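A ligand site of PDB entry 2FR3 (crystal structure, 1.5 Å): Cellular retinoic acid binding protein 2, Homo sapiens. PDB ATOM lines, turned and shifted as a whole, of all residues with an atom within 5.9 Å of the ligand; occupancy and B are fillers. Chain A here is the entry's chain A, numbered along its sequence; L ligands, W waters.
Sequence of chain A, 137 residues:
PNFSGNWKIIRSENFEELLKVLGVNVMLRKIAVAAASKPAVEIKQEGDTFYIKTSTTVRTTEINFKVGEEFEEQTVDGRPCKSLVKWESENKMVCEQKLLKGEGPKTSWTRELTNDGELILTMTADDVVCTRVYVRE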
ATOM      1  N   ILE A   9       4.688   7.643 -34.367  1.00  0.00           N
ATOM      2  CA  ILE A   9       3.291   7.747 -33.992  1.00  0.00           C
ATOM      3  C   ILE A   9       2.413   8.267 -35.122  1.00  0.00           C
ATOM      4  O   ILE A   9       2.822   9.208 -35.824  1.00  0.00           O
ATOM      5  CB  ILE A   9       3.096   8.578 -32.688  1.00  0.00           C
ATOM      6  CG1 ILE A   9       1.726   8.289 -32.055  1.00  0.00           C
ATOM      7  CG2 ILE A   9       3.307  10.019 -32.938  1.00  0.00           C
ATOM      8  CD1 ILE A   9       1.622   8.715 -30.603  1.00  0.00           C
ATOM      9  N   PHE A  15      -4.723  10.498 -24.183  1.00  0.00           N
ATOM     10  CA  PHE A  15      -3.512  10.609 -23.342  1.00  0.00           C
ATOM     11  C   PHE A  15      -3.688  11.670 -22.269  1.00  0.00           C
ATOM     12  O   PHE A  15      -3.333  11.445 -21.098  1.00  0.00           O
ATOM     13  CB  PHE A  15      -2.296  10.893 -24.214  1.00  0.00           C
ATOM     14  CG  PHE A  15      -0.977  10.922 -23.473  1.00  0.00           C
ATOM     15  CD1 PHE A  15      -0.559   9.849 -22.736  1.00  0.00           C
ATOM     16  CD2 PHE A  15      -0.186  12.051 -23.464  1.00  0.00           C
ATOM     17  CE1 PHE A  15       0.655   9.896 -22.034  1.00  0.00           C
ATOM     18  CE2 PHE A  15       0.996  12.067 -22.770  1.00  0.00           C
ATOM     19  CZ  PHE A  15       1.398  11.011 -22.101  1.00  0.00           C
ATOM     20  N   LEU A  19      -3.685  11.125 -18.092  1.00  0.00           N
ATOM     21  CA  LEU A  19      -2.855  11.917 -17.133  1.00  0.00           C
ATOM     22  C   LEU A  19      -3.741  12.583 -16.073  1.00  0.00           C
ATOM     23  O   LEU A  19      -3.333  12.701 -14.920  1.00  0.00           O
ATOM     24  CB  LEU A  19      -1.998  12.957 -17.848  1.00  0.00           C
ATOM     25  CG  LEU A  19      -0.990  12.329 -18.808  1.00  0.00           C
ATOM     26  CD1 LEU A  19      -0.090  13.412 -19.388  1.00  0.00           C
ATOM     27  CD2 LEU A  19      -0.106  11.267 -18.187  1.00  0.00           C
ATOM     28  N   VAL A  24      -2.139  14.346 -12.688  1.00  0.00           N
ATOM     29  CA  VAL A  24      -1.215  15.301 -13.206  1.00  0.00           C
ATOM     30  C   VAL A  24      -1.933  16.631 -13.474  1.00  0.00           C
ATOM     31  O   VAL A  24      -2.932  16.673 -14.192  1.00  0.00           O
ATOM     32  CB  VAL A  24      -0.545  14.767 -14.530  1.00  0.00           C
ATOM     33  CG1 VAL A  24       0.473  15.779 -15.083  1.00  0.00           C
ATOM     34  CG2 VAL A  24       0.056  13.396 -14.261  1.00  0.00           C
ATOM     35  N   LEU A  28       1.305  20.664 -16.248  1.00  0.00           N
ATOM     36  CA  LEU A  28       2.162  19.494 -16.543  1.00  0.00           C
ATOM     37  C   LEU A  28       1.560  18.669 -17.637  1.00  0.00           C
ATOM     38  O   LEU A  28       2.302  18.161 -18.470  1.00  0.00           O
ATOM     39  CB  LEU A  28       2.396  18.622 -15.311  1.00  0.00           C
ATOM     40  CG  LEU A  28       3.304  19.269 -14.290  1.00  0.00           C
ATOM     41  CD1 LEU A  28       3.222  18.500 -12.983  1.00  0.00           C
ATOM     42  CD2 LEU A  28       4.724  19.349 -14.698  1.00  0.00           C
ATOM     43  N   ILE A  31       2.532  20.244 -21.019  1.00  0.00           N
ATOM     44  CA  ILE A  31       3.916  19.963 -21.316  1.00  0.00           C
ATOM     45  C   ILE A  31       3.976  18.512 -21.870  1.00  0.00           C
ATOM     46  O   ILE A  31       4.597  18.223 -22.914  1.00  0.00           O
ATOM     47  CB  ILE A  31       4.865  20.123 -20.067  1.00  0.00           C
ATOM     48  CG1 ILE A  31       4.875  21.609 -19.623  1.00  0.00           C
ATOM     49  CG2 ILE A  31       6.239  19.565 -20.361  1.00  0.00           C
ATOM     50  CD1 ILE A  31       5.393  21.841 -18.198  1.00  0.00           C
ATOM     51  N   ALA A  32       3.395  17.592 -21.106  1.00  0.00           N
ATOM     52  CA  ALA A  32       3.494  16.170 -21.485  1.00  0.00           C
ATOM     53  C   ALA A  32       2.836  15.805 -22.804  1.00  0.00           C
ATOM     54  O   ALA A  32       3.405  15.088 -23.599  1.00  0.00           O
ATOM     55  CB  ALA A  32       2.929  15.305 -20.390  1.00  0.00           C
ATOM     56  N   VAL A  33       1.656  16.332 -23.026  1.00  0.00           N
ATOM     57  CA  VAL A  33       0.924  16.015 -24.263  1.00  0.00           C
ATOM     58  C   VAL A  33       1.685  16.519 -25.456  1.00  0.00           C
ATOM     59  O   VAL A  33       1.829  15.816 -26.467  1.00  0.00           O
ATOM     60  CB  VAL A  33      -0.534  16.517 -24.240  1.00  0.00           C
ATOM     61  CG1 VAL A  33      -1.175  16.206 -25.539  1.00  0.00           C
ATOM     62  CG2 VAL A  33      -1.311  15.826 -23.157  1.00  0.00           C
ATOM     63  N   ALA A  35       4.936  17.086 -25.759  1.00  0.00           N
ATOM     64  CA  ALA A  35       6.152  16.340 -25.943  1.00  0.00           C
ATOM     65  C   ALA A  35       5.849  14.938 -26.476  1.00  0.00           C
ATOM     66  O   ALA A  35       6.564  14.395 -27.304  1.00  0.00           O
ATOM     67  CB  ALA A  35       6.933  16.259 -24.641  1.00  0.00           C
ATOM     68  N   ALA A  36       4.787  14.338 -25.964  1.00  0.00           N
ATOM     69  CA  ALA A  36       4.404  12.989 -26.360  1.00  0.00           C
ATOM     70  C   ALA A  36       3.823  12.928 -27.760  1.00  0.00           C
ATOM     71  O   ALA A  36       3.644  11.838 -28.289  1.00  0.00           O
ATOM     72  CB  ALA A  36       3.405  12.415 -25.321  1.00  0.00           C
ATOM     73  N   PRO A  39       7.134  11.337 -30.262  1.00  0.00           N
ATOM     74  CA  PRO A  39       8.123  10.531 -29.634  1.00  0.00           C
ATOM     75  C   PRO A  39       8.993   9.798 -30.621  1.00  0.00           C
ATOM     76  O   PRO A  39       8.558   9.573 -31.762  1.00  0.00           O
ATOM     77  CB  PRO A  39       7.302   9.536 -28.862  1.00  0.00           C
ATOM     78  CG  PRO A  39       6.107   9.338 -29.740  1.00  0.00           C
ATOM     79  CD  PRO A  39       5.819  10.655 -30.332  1.00  0.00           C
ATOM     80  N   VAL A  41      10.516   5.995 -30.718  1.00  0.00           N
ATOM     81  CA  VAL A  41      10.347   4.713 -30.076  1.00  0.00           C
ATOM     82  C   VAL A  41      11.205   3.676 -30.773  1.00  0.00           C
ATOM     83  O   VAL A  41      11.038   3.453 -31.970  1.00  0.00           O
ATOM     84  CB  VAL A  41       8.826   4.242 -30.126  1.00  0.00           C
ATOM     85  CG1 VAL A  41       8.659   2.874 -29.564  1.00  0.00           C
ATOM     86  CG2 VAL A  41       7.957   5.272 -29.361  1.00  0.00           C
ATOM     87  N   THR A  54      11.740   4.823 -25.224  1.00  0.00           N
ATOM     88  CA  THR A  54      10.766   5.817 -25.676  1.00  0.00           C
ATOM     89  C   THR A  54      11.290   7.189 -25.291  1.00  0.00           C
ATOM     90  O   THR A  54      11.476   7.448 -24.086  1.00  0.00           O
ATOM     91  CB  THR A  54       9.418   5.598 -25.021  1.00  0.00           C
ATOM     92  OG1 THR A  54       8.935   4.288 -25.348  1.00  0.00           O
ATOM     93  CG2 THR A  54       8.424   6.672 -25.469  1.00  0.00           C
ATOM     94  N   SER A  55      11.548   8.047 -26.276  1.00  0.00           N
ATOM     95  CA  SER A  55      12.220   9.317 -26.073  1.00  0.00           C
ATOM     96  C   SER A  55      11.328  10.476 -26.479  1.00  0.00           C
ATOM     97  O   SER A  55      10.707  10.482 -27.540  1.00  0.00           O
ATOM     98  CB  SER A  55      13.499   9.434 -26.928  1.00  0.00           C
ATOM     99  OG  SER A  55      14.429   8.387 -26.735  1.00  0.00           O
ATOM    100  N   THR A  56      11.281  11.474 -25.602  1.00  0.00           N
ATOM    101  CA  THR A  56      10.659  12.755 -25.882  1.00  0.00           C
ATOM    102  C   THR A  56      11.572  13.862 -25.355  1.00  0.00           C
ATOM    103  O   THR A  56      12.523  13.581 -24.653  1.00  0.00           O
ATOM    104  CB  THR A  56       9.293  12.918 -25.207  1.00  0.00           C
ATOM    105  OG1 THR A  56       9.425  13.107 -23.812  1.00  0.00           O
ATOM    106  CG2 THR A  56       8.356  11.765 -25.505  1.00  0.00           C
ATOM    107  N   VAL A  58      11.086  15.811 -22.977  1.00  0.00           N
ATOM    108  CA  VAL A  58      10.867  16.020 -21.542  1.00  0.00           C
ATOM    109  C   VAL A  58      11.044  14.804 -20.681  1.00  0.00           C
ATOM    110  O   VAL A  58      11.052  14.906 -19.463  1.00  0.00           O
ATOM    111  CB  VAL A  58       9.492  16.625 -21.212  1.00  0.00           C
ATOM    112  CG1 VAL A  58       9.272  17.897 -21.988  1.00  0.00           C
ATOM    113  CG2 VAL A  58       8.361  15.703 -21.483  1.00  0.00           C
ATOM    114  N   ARG A  59      11.196  13.632 -21.304  1.00  0.00           N
ATOM    115  CA  ARG A  59      11.301  12.371 -20.588  1.00  0.00           C
ATOM    116  C   ARG A  59      11.698  11.303 -21.557  1.00  0.00           C
ATOM    117  O   ARG A  59      11.124  11.180 -22.642  1.00  0.00           O
ATOM    118  CB  ARG A  59       9.985  12.024 -19.908  1.00  0.00           C
ATOM    119  CG  ARG A  59       9.930  10.756 -19.135  1.00  0.00           C
ATOM    120  CD  ARG A  59       8.570  10.711 -18.310  1.00  0.00           C
ATOM    121  NE  ARG A  59       8.255   9.364 -17.885  1.00  0.00           N
ATOM    122  CZ  ARG A  59       8.728   8.765 -16.793  1.00  0.00           C
ATOM    123  NH1 ARG A  59       9.552   9.398 -15.959  1.00  0.00           N
ATOM    124  NH2 ARG A  59       8.416   7.491 -16.531  1.00  0.00           N
ATOM    125  N   VAL A  76       3.379   5.591 -16.292  1.00  0.00           N
ATOM    126  CA  VAL A  76       3.462   6.668 -17.232  1.00  0.00           C
ATOM    127  C   VAL A  76       3.672   8.040 -16.553  1.00  0.00           C
ATOM    128  O   VAL A  76       4.354   8.911 -17.095  1.00  0.00           O
ATOM    129  CB  VAL A  76       2.233   6.570 -18.182  1.00  0.00           C
ATOM    130  CG1 VAL A  76       0.999   6.842 -17.427  1.00  0.00           C
ATOM    131  CG2 VAL A  76       2.463   7.544 -19.370  1.00  0.00           C
ATOM    132  N   ASP A  77       3.142   8.203 -15.350  1.00  0.00           N
ATOM    133  CA  ASP A  77       3.295   9.447 -14.567  1.00  0.00           C
ATOM    134  C   ASP A  77       4.515   9.428 -13.656  1.00  0.00           C
ATOM    135  O   ASP A  77       4.709  10.341 -12.860  1.00  0.00           O
ATOM    136  CB  ASP A  77       2.002   9.791 -13.796  1.00  0.00           C
ATOM    137  CG  ASP A  77       1.610   8.748 -12.770  1.00  0.00           C
ATOM    138  OD1 ASP A  77       1.570   7.540 -13.122  1.00  0.00           O
ATOM    139  OD2 ASP A  77       1.305   9.121 -11.617  1.00  0.00           O
ATOM    140  N   GLY A  78       5.353   8.433 -13.835  1.00  0.00           N
ATOM    141  CA  GLY A  78       6.699   8.516 -13.291  1.00  0.00           C
ATOM    142  C   GLY A  78       6.926   7.876 -11.958  1.00  0.00           C
ATOM    143  O   GLY A  78       7.947   8.126 -11.344  1.00  0.00           O
ATOM    144  N   ARG A 111       0.782  -3.915 -25.677  1.00  0.00           N
ATOM    145  CA  ARG A 111       1.323  -3.634 -26.998  1.00  0.00           C
ATOM    146  C   ARG A 111       0.952  -4.753 -27.948  1.00  0.00           C
ATOM    147  O   ARG A 111       1.130  -5.912 -27.612  1.00  0.00           O
ATOM    148  CB  ARG A 111       2.825  -3.473 -26.972  1.00  0.00           C
ATOM    149  CG  ARG A 111       3.231  -2.098 -26.435  1.00  0.00           C
ATOM    150  CD  ARG A 111       4.748  -1.892 -26.422  1.00  0.00           C
ATOM    151  NE  ARG A 111       5.168  -0.524 -26.106  1.00  0.00           N
ATOM    152  CZ  ARG A 111       5.507  -0.090 -24.906  1.00  0.00           C
ATOM    153  NH1 ARG A 111       5.500  -0.860 -23.826  1.00  0.00           N
ATOM    154  NH2 ARG A 111       5.894   1.195 -24.804  1.00  0.00           N
ATOM    155  N   LEU A 121      -0.281   0.670 -28.807  1.00  0.00           N
ATOM    156  CA  LEU A 121       0.009   0.728 -27.395  1.00  0.00           C
ATOM    157  C   LEU A 121      -1.266   1.171 -26.725  1.00  0.00           C
ATOM    158  O   LEU A 121      -1.867   2.170 -27.141  1.00  0.00           O
ATOM    159  CB  LEU A 121       1.101   1.786 -27.079  1.00  0.00           C
ATOM    160  CG  LEU A 121       1.287   2.190 -25.619  1.00  0.00           C
ATOM    161  CD1 LEU A 121       1.881   1.018 -24.785  1.00  0.00           C
ATOM    162  CD2 LEU A 121       2.213   3.415 -25.502  1.00  0.00           C
ATOM    163  N   MET A 123      -2.534   2.244 -22.711  1.00  0.00           N
ATOM    164  CA  MET A 123      -2.179   2.526 -21.328  1.00  0.00           C
ATOM    165  C   MET A 123      -3.450   2.774 -20.576  1.00  0.00           C
ATOM    166  O   MET A 123      -4.273   3.549 -21.029  1.00  0.00           O
ATOM    167  CB  MET A 123      -1.227   3.697 -21.180  1.00  0.00           C
ATOM    168  CG  MET A 123       0.117   3.443 -21.841  1.00  0.00           C
ATOM    169  SD  MET A 123       1.212   4.870 -21.755  1.00  0.00           S
ATOM    170  CE  MET A 123       0.520   5.936 -22.930  1.00  0.00           C
ATOM    171  N   ARG A 132      -2.607   4.498 -28.565  1.00  0.00           N
ATOM    172  CA  ARG A 132      -1.632   5.121 -29.417  1.00  0.00           C
ATOM    173  C   ARG A 132      -1.257   4.141 -30.492  1.00  0.00           C
ATOM    174  O   ARG A 132      -1.057   2.959 -30.206  1.00  0.00           O
ATOM    175  CB  ARG A 132      -0.465   5.664 -28.628  1.00  0.00           C
ATOM    176  CG  ARG A 132      -0.839   6.959 -27.877  1.00  0.00           C
ATOM    177  CD  ARG A 132       0.054   7.220 -26.680  1.00  0.00           C
ATOM    178  NE  ARG A 132       1.391   7.638 -27.093  1.00  0.00           N
ATOM    179  CZ  ARG A 132       1.740   8.914 -27.292  1.00  0.00           C
ATOM    180  NH1 ARG A 132       0.857   9.880 -27.252  1.00  0.00           N
ATOM    181  NH2 ARG A 132       2.998   9.205 -27.605  1.00  0.00           N
ATOM    182  N   TYR A 134       1.217   3.291 -33.994  1.00  0.00           N
ATOM    183  CA  TYR A 134       2.499   3.582 -34.597  1.00  0.00           C
ATOM    184  C   TYR A 134       2.674   2.716 -35.842  1.00  0.00           C
ATOM    185  O   TYR A 134       2.091   1.651 -35.993  1.00  0.00           O
ATOM    186  CB  TYR A 134       3.676   3.223 -33.665  1.00  0.00           C
ATOM    187  CG  TYR A 134       3.590   3.819 -32.295  1.00  0.00           C
ATOM    188  CD1 TYR A 134       2.706   3.296 -31.368  1.00  0.00           C
ATOM    189  CD2 TYR A 134       4.359   4.888 -31.938  1.00  0.00           C
ATOM    190  CE1 TYR A 134       2.559   3.812 -30.115  1.00  0.00           C
ATOM    191  CE2 TYR A 134       4.201   5.420 -30.611  1.00  0.00           C
ATOM    192  CZ  TYR A 134       3.295   4.852 -29.725  1.00  0.00           C
ATOM    193  OH  TYR A 134       3.103   5.323 -28.403  1.00  0.00           O
HETATM  194  C1  LIG L   1       6.208  15.156 -17.354  1.00  0.00           C
HETATM  195  C2  LIG L   1       6.123  15.389 -15.851  1.00  0.00           C
HETATM  196  C3  LIG L   1       4.699  15.230 -15.338  1.00  0.00           C
HETATM  197  C4  LIG L   1       4.241  13.817 -15.532  1.00  0.00           C
HETATM  198  C5  LIG L   1       4.320  13.453 -16.981  1.00  0.00           C
HETATM  199  C6  LIG L   1       5.314  14.019 -17.808  1.00  0.00           C
HETATM  200  C7  LIG L   1       5.659  13.605 -19.163  1.00  0.00           C
HETATM  201  C8  LIG L   1       5.405  12.309 -19.614  1.00  0.00           C
HETATM  202  C9  LIG L   1       5.599  11.953 -21.014  1.00  0.00           C
HETATM  203  C10 LIG L   1       5.243  10.622 -21.363  1.00  0.00           C
HETATM  204  C11 LIG L   1       5.255  10.234 -22.759  1.00  0.00           C
HETATM  205  C12 LIG L   1       4.752   8.908 -23.038  1.00  0.00           C
HETATM  206  C13 LIG L   1       4.888   8.378 -24.370  1.00  0.00           C
HETATM  207  C14 LIG L   1       4.237   7.172 -24.544  1.00  0.00           C
HETATM  208  C15 LIG L   1       4.487   6.356 -25.718  1.00  0.00           C
HETATM  209  C16 LIG L   1       7.660  14.787 -17.675  1.00  0.00           C
HETATM  210  C17 LIG L   1       5.913  16.423 -18.141  1.00  0.00           C
HETATM  211  C18 LIG L   1       3.265  12.549 -17.492  1.00  0.00           C
HETATM  212  C19 LIG L   1       6.058  12.903 -22.057  1.00  0.00           C
HETATM  213  C20 LIG L   1       5.717   9.072 -25.398  1.00  0.00           C
HETATM  214  O1  LIG L   1       4.245   6.816 -26.858  1.00  0.00           O
HETATM  215  O2  LIG L   1       4.879   5.209 -25.588  1.00  0.00           O
HETATM  216  O   HOH W   1       6.570  11.130 -16.168  1.00  0.00           O
HETATM  217  O   HOH W   2       5.712   4.428 -23.121  1.00  0.00           O
HETATM  218  O   HOH W   3       6.355   3.389 -26.639  1.00  0.00           O
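N of Val 58 sits close to OG1 of Thr 56 (3.3 Å).
The backbone NH (N) of Val 24 lies within hydrogen-bond range of the backbone carbonyl oxygen (O) of Leu 19 (3.0 Å).
NH2 of Arg 132 is in hydrogen-bond range of O of Ala 36, at 2.8 Å.
OG1 of Thr 56 is in hydrogen-bond range of O of Arg 59 (2.8 Å).
O of Arg 132 sits at hydrogen-bond distance from N of Leu 121.
OH of Tyr 134 lies within hydrogen-bond range of NE of Arg 132 (3.2 Å).
Phe 15 touches the ligand.
CD2 of Leu 19 touches C18 of the ligand (3.7 Å).
Ile 31 touches the ligand (CG2 to C17, 3.9 Å).
Ala 32 touches the ligand.
CB of Ala 36 touches C11 of the ligand, 3.8 Å away.
Pro 39 touches the ligand (CB to C20, 3.8 Å).
Thr 54 touches the ligand.
Thr 56 touches the ligand.
Val 58 touches the ligand (CG2 to C19, 3.7 Å).
CD of Arg 59 touches C8 of the ligand (3.8 Å).
Val 76 touches the ligand.
CD2 of Leu 121 touches O2 of the ligand, at 3.2 Å.
Hydrophobic or aromatic side chains that line the ligand: Phe 15, Leu 19, Ile 31, Ala 32, Ala 36, Pro 39, Val 58, Leu 121 and Tyr 134.
Within 4 Å of the ligand: Phe 15, Leu 19, Ile 31, Ala 32, Ala 36, Pro 39, Thr 54, Thr 56, Val 58, Arg 59, Val 76, Leu 121, Arg 132 and Tyr 134.
Water W3 lies within hydrogen-bond range of O2 of the ligand, NH2 of Arg 111 and OG1 of Thr 54.
Water W1 lies within hydrogen-bond range of the guanidinium group of Arg 59 (3.0 Å) and the backbone carbonyl oxygen of Val 76 (3.3 Å).
The guanidinium group (NH2) of Arg 132 lies within salt-bridge range of an oxygen (O1) of the ligand (2.8 Å).
An oxygen (O1) of the ligand sits at hydrogen-bond distance from the side-chain hydroxyl (OH) of Tyr 134, 2.4 Å away.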
